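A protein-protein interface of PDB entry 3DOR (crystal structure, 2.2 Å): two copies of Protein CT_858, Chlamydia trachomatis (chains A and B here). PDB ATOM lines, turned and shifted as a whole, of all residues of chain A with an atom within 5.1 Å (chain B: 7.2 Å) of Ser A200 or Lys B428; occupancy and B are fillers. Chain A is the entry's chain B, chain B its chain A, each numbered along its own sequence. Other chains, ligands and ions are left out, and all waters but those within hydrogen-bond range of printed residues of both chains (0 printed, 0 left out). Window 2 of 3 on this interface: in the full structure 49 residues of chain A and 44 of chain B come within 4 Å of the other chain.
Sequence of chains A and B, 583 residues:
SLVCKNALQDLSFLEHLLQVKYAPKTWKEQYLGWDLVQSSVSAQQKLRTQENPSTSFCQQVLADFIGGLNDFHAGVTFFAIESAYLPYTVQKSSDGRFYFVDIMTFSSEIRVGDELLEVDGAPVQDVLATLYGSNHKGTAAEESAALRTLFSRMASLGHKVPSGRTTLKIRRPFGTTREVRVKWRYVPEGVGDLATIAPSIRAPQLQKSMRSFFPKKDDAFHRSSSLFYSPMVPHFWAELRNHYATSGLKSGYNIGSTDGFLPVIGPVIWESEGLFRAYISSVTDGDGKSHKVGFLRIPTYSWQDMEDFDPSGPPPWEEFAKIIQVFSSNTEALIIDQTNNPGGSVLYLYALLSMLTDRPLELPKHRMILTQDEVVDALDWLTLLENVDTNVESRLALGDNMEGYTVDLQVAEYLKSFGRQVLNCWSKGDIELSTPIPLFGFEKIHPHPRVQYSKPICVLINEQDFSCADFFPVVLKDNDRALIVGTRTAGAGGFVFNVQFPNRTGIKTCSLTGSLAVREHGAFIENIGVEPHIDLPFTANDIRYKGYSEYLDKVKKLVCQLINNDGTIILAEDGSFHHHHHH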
ATOM      1  N   ILE A 197       6.754  27.594 -12.502  1.00  0.00           N
ATOM      2  CA  ILE A 197       8.070  27.065 -12.833  1.00  0.00           C
ATOM      3  C   ILE A 197       9.144  28.136 -13.011  1.00  0.00           C
ATOM      4  O   ILE A 197      10.320  27.884 -12.771  1.00  0.00           O
ATOM      5  CB  ILE A 197       7.978  26.225 -14.123  1.00  0.00           C
ATOM      6  CG1 ILE A 197       6.981  25.081 -13.917  1.00  0.00           C
ATOM      7  CG2 ILE A 197       9.338  25.689 -14.500  1.00  0.00           C
ATOM      8  CD1 ILE A 197       6.660  24.307 -15.181  1.00  0.00           C
ATOM      9  N   ALA A 198       8.731  29.327 -13.425  1.00  0.00           N
ATOM     10  CA  ALA A 198       9.644  30.444 -13.680  1.00  0.00           C
ATOM     11  C   ALA A 198      10.809  30.639 -12.700  1.00  0.00           C
ATOM     12  O   ALA A 198      11.971  30.670 -13.111  1.00  0.00           O
ATOM     13  CB  ALA A 198       8.850  31.736 -13.793  1.00  0.00           C
ATOM     14  N   PRO A 199      10.517  30.780 -11.396  1.00  0.00           N
ATOM     15  CA  PRO A 199      11.593  30.977 -10.417  1.00  0.00           C
ATOM     16  C   PRO A 199      12.724  29.943 -10.432  1.00  0.00           C
ATOM     17  O   PRO A 199      13.857  30.261 -10.072  1.00  0.00           O
ATOM     18  CB  PRO A 199      10.845  31.009  -9.081  1.00  0.00           C
ATOM     19  CG  PRO A 199       9.625  30.167  -9.347  1.00  0.00           C
ATOM     20  CD  PRO A 199       9.214  30.645 -10.716  1.00  0.00           C
ATOM     21  N   SER A 200      12.429  28.716 -10.849  1.00  0.00           N
ATOM     22  CA  SER A 200      13.452  27.675 -10.877  1.00  0.00           C
ATOM     23  C   SER A 200      14.115  27.480 -12.243  1.00  0.00           C
ATOM     24  O   SER A 200      14.867  26.527 -12.437  1.00  0.00           O
ATOM     25  CB  SER A 200      12.860  26.344 -10.405  1.00  0.00           C
ATOM     26  OG  SER A 200      11.870  25.875 -11.300  1.00  0.00           O
ATOM     27  N   ILE A 201      13.840  28.377 -13.186  1.00  0.00           N
ATOM     28  CA  ILE A 201      14.430  28.272 -14.518  1.00  0.00           C
ATOM     29  C   ILE A 201      15.828  28.883 -14.549  1.00  0.00           C
ATOM     30  O   ILE A 201      15.990  30.094 -14.406  1.00  0.00           O
ATOM     31  CB  ILE A 201      13.570  28.983 -15.587  1.00  0.00           C
ATOM     32  CG1 ILE A 201      12.216  28.282 -15.724  1.00  0.00           C
ATOM     33  CG2 ILE A 201      14.305  28.986 -16.925  1.00  0.00           C
ATOM     34  CD1 ILE A 201      11.290  28.935 -16.732  1.00  0.00           C
ATOM     35  N   ARG A 202      16.835  28.041 -14.749  1.00  0.00           N
ATOM     36  CA  ARG A 202      18.211  28.511 -14.793  1.00  0.00           C
ATOM     37  C   ARG A 202      18.709  28.626 -16.230  1.00  0.00           C
ATOM     38  O   ARG A 202      18.153  28.013 -17.146  1.00  0.00           O
ATOM     39  CB  ARG A 202      19.112  27.556 -14.008  1.00  0.00           C
ATOM     40  CG  ARG A 202      18.586  27.224 -12.620  1.00  0.00           C
ATOM     41  CD  ARG A 202      19.645  26.547 -11.766  1.00  0.00           C
ATOM     42  NE  ARG A 202      19.113  26.128 -10.471  1.00  0.00           N
ATOM     43  CZ  ARG A 202      19.855  25.656  -9.472  1.00  0.00           C
ATOM     44  NH1 ARG A 202      21.171  25.545  -9.615  1.00  0.00           N
ATOM     45  NH2 ARG A 202      19.282  25.288  -8.332  1.00  0.00           N
ATOM     46  N   VAL B 422      10.484  14.173 -19.670  1.00  0.00           N
ATOM     47  CA  VAL B 422      10.161  15.489 -20.212  1.00  0.00           C
ATOM     48  C   VAL B 422       9.336  16.257 -19.183  1.00  0.00           C
ATOM     49  O   VAL B 422       9.584  17.437 -18.927  1.00  0.00           O
ATOM     50  CB  VAL B 422       9.361  15.373 -21.535  1.00  0.00           C
ATOM     51  CG1 VAL B 422       8.889  16.748 -21.994  1.00  0.00           C
ATOM     52  CG2 VAL B 422      10.230  14.736 -22.609  1.00  0.00           C
ATOM     53  N   LEU B 423       8.354  15.579 -18.594  1.00  0.00           N
ATOM     54  CA  LEU B 423       7.500  16.199 -17.587  1.00  0.00           C
ATOM     55  C   LEU B 423       8.332  16.595 -16.368  1.00  0.00           C
ATOM     56  O   LEU B 423       8.131  17.656 -15.777  1.00  0.00           O
ATOM     57  CB  LEU B 423       6.385  15.234 -17.172  1.00  0.00           C
ATOM     58  CG  LEU B 423       5.310  14.973 -18.237  1.00  0.00           C
ATOM     59  CD1 LEU B 423       4.349  13.895 -17.762  1.00  0.00           C
ATOM     60  CD2 LEU B 423       4.552  16.269 -18.531  1.00  0.00           C
ATOM     61  N   ASN B 424       9.278  15.739 -16.004  1.00  0.00           N
ATOM     62  CA  ASN B 424      10.132  16.016 -14.862  1.00  0.00           C
ATOM     63  C   ASN B 424      10.951  17.276 -15.133  1.00  0.00           C
ATOM     64  O   ASN B 424      11.038  18.162 -14.282  1.00  0.00           O
ATOM     65  CB  ASN B 424      11.061  14.830 -14.602  1.00  0.00           C
ATOM     66  CG  ASN B 424      11.723  14.900 -13.244  1.00  0.00           C
ATOM     67  OD1 ASN B 424      12.313  15.916 -12.881  1.00  0.00           O
ATOM     68  ND2 ASN B 424      11.632  13.813 -12.484  1.00  0.00           N
ATOM     69  N   CYS B 425      11.540  17.359 -16.325  1.00  0.00           N
ATOM     70  CA  CYS B 425      12.348  18.517 -16.705  1.00  0.00           C
ATOM     71  C   CYS B 425      11.536  19.805 -16.710  1.00  0.00           C
ATOM     72  O   CYS B 425      12.038  20.868 -16.338  1.00  0.00           O
ATOM     73  CB  CYS B 425      12.960  18.311 -18.093  1.00  0.00           C
ATOM     74  SG  CYS B 425      14.178  16.981 -18.195  1.00  0.00           S
ATOM     75  N   TRP B 426      10.284  19.709 -17.149  1.00  0.00           N
ATOM     76  CA  TRP B 426       9.401  20.867 -17.209  1.00  0.00           C
ATOM     77  C   TRP B 426       9.086  21.373 -15.804  1.00  0.00           C
ATOM     78  O   TRP B 426       9.234  22.563 -15.518  1.00  0.00           O
ATOM     79  CB  TRP B 426       8.108  20.502 -17.954  1.00  0.00           C
ATOM     80  CG  TRP B 426       7.114  21.628 -18.084  1.00  0.00           C
ATOM     81  CD1 TRP B 426       5.935  21.763 -17.405  1.00  0.00           C
ATOM     82  CD2 TRP B 426       7.210  22.770 -18.947  1.00  0.00           C
ATOM     83  NE1 TRP B 426       5.290  22.916 -17.794  1.00  0.00           N
ATOM     84  CE2 TRP B 426       6.051  23.552 -18.740  1.00  0.00           C
ATOM     85  CE3 TRP B 426       8.162  23.205 -19.877  1.00  0.00           C
ATOM     86  CZ2 TRP B 426       5.819  24.748 -19.422  1.00  0.00           C
ATOM     87  CZ3 TRP B 426       7.934  24.395 -20.558  1.00  0.00           C
ATOM     88  CH2 TRP B 426       6.767  25.152 -20.326  1.00  0.00           C
ATOM     89  N   SER B 427       8.667  20.470 -14.926  1.00  0.00           N
ATOM     90  CA  SER B 427       8.345  20.859 -13.561  1.00  0.00           C
ATOM     91  C   SER B 427       9.571  21.406 -12.838  1.00  0.00           C
ATOM     92  O   SER B 427       9.450  22.267 -11.966  1.00  0.00           O
ATOM     93  CB  SER B 427       7.767  19.669 -12.786  1.00  0.00           C
ATOM     94  OG  SER B 427       8.627  18.547 -12.841  1.00  0.00           O
ATOM     95  N   LYS B 428      10.751  20.913 -13.202  1.00  0.00           N
ATOM     96  CA  LYS B 428      11.985  21.375 -12.576  1.00  0.00           C
ATOM     97  C   LYS B 428      12.469  22.687 -13.166  1.00  0.00           C
ATOM     98  O   LYS B 428      13.393  23.304 -12.644  1.00  0.00           O
ATOM     99  CB  LYS B 428      13.095  20.333 -12.726  1.00  0.00           C
ATOM    100  CG  LYS B 428      12.970  19.135 -11.803  1.00  0.00           C
ATOM    101  CD  LYS B 428      14.167  18.216 -11.960  1.00  0.00           C
ATOM    102  CE  LYS B 428      14.085  17.034 -11.009  1.00  0.00           C
ATOM    103  NZ  LYS B 428      15.226  16.094 -11.191  1.00  0.00           N
ATOM    104  N   GLY B 429      11.854  23.112 -14.263  1.00  0.00           N
ATOM    105  CA  GLY B 429      12.273  24.353 -14.887  1.00  0.00           C
ATOM    106  C   GLY B 429      13.492  24.170 -15.773  1.00  0.00           C
ATOM    107  O   GLY B 429      14.061  25.142 -16.272  1.00  0.00           O
ATOM    108  N   ASP B 430      13.902  22.918 -15.958  1.00  0.00           N
ATOM    109  CA  ASP B 430      15.051  22.577 -16.799  1.00  0.00           C
ATOM    110  C   ASP B 430      14.507  22.545 -18.231  1.00  0.00           C
ATOM    111  O   ASP B 430      14.336  21.475 -18.821  1.00  0.00           O
ATOM    112  CB  ASP B 430      15.589  21.203 -16.372  1.00  0.00           C
ATOM    113  CG  ASP B 430      16.765  20.731 -17.213  1.00  0.00           C
ATOM    114  OD1 ASP B 430      17.643  21.553 -17.549  1.00  0.00           O
ATOM    115  OD2 ASP B 430      16.816  19.523 -17.517  1.00  0.00           O
ATOM    116  N   ILE B 431      14.243  23.730 -18.780  1.00  0.00           N
ATOM    117  CA  ILE B 431      13.654  23.851 -20.110  1.00  0.00           C
ATOM    118  C   ILE B 431      14.438  24.610 -21.178  1.00  0.00           C
ATOM    119  O   ILE B 431      14.058  24.583 -22.347  1.00  0.00           O
ATOM    120  CB  ILE B 431      12.262  24.497 -20.013  1.00  0.00           C
ATOM    121  CG1 ILE B 431      12.395  25.947 -19.546  1.00  0.00           C
ATOM    122  CG2 ILE B 431      11.400  23.719 -19.031  1.00  0.00           C
ATOM    123  CD1 ILE B 431      11.077  26.706 -19.508  1.00  0.00           C
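The backbone carbonyl oxygen (O) of Lys B428 lies within hydrogen-bond range of the side-chain hydroxyl (OG) of Ser A200, 3.3 Å away.
The side-chain amino group (NZ) of Lys B428 lies close to the side-chain amide oxygen (OD1) of Asn B424. The backbone carbonyl oxygen (O) of Ile A197 is in hydrogen-bond range of the side-chain hydroxyl (OG) of Ser A200 (2.9 Å).
Ile A197 touches Trp B426. Ile A197 touches Gly B429 (CG2 to CA, 3.2 Å). OG of Ser A200 touches CA of Gly B429, 3.9 Å away. Ile A201 touches Gly B429. Ile A201 touches Ile B431.
Of chain B, only Lys B428 (3.3 Å) and Gly B429 (3.9 Å) come within 4 Å of Ser A200. Of chain A, only Ser A200 comes within 4 Å of Lys B428. Printed residues of chain A within 4 Å of Ile B431: Ile A201 (3.6 Å). Of the printed residues of chain A, Trp B426 touches Ile A197. Of the printed residues of chain B, Ile A197 touches Trp B426 (3.1 Å) and Gly B429 (3.2 Å). Asp B430 touches none of the printed residues of chain A. Cys B425 touches none of the printed residues of chain A. The nearest residue of chain A that does not touch Lys B428 is Ile A197 (4.5 Å). The nearest printed residue of chain A that does not touch Gly B429 is Arg A202 (4.3 Å).
Of the 10 printed residues of chain B, 4 touch a printed residue of chain A. Hydrophobic or aromatic side chains of chain B that line the printed part of chain A: Trp B426 and Ile B431. Along chain A the printed residues that touch a printed residue of chain B span positions 197 to 201. Among the printed residues, 6 pairs touch across the chains.
No position is printed for both chains.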
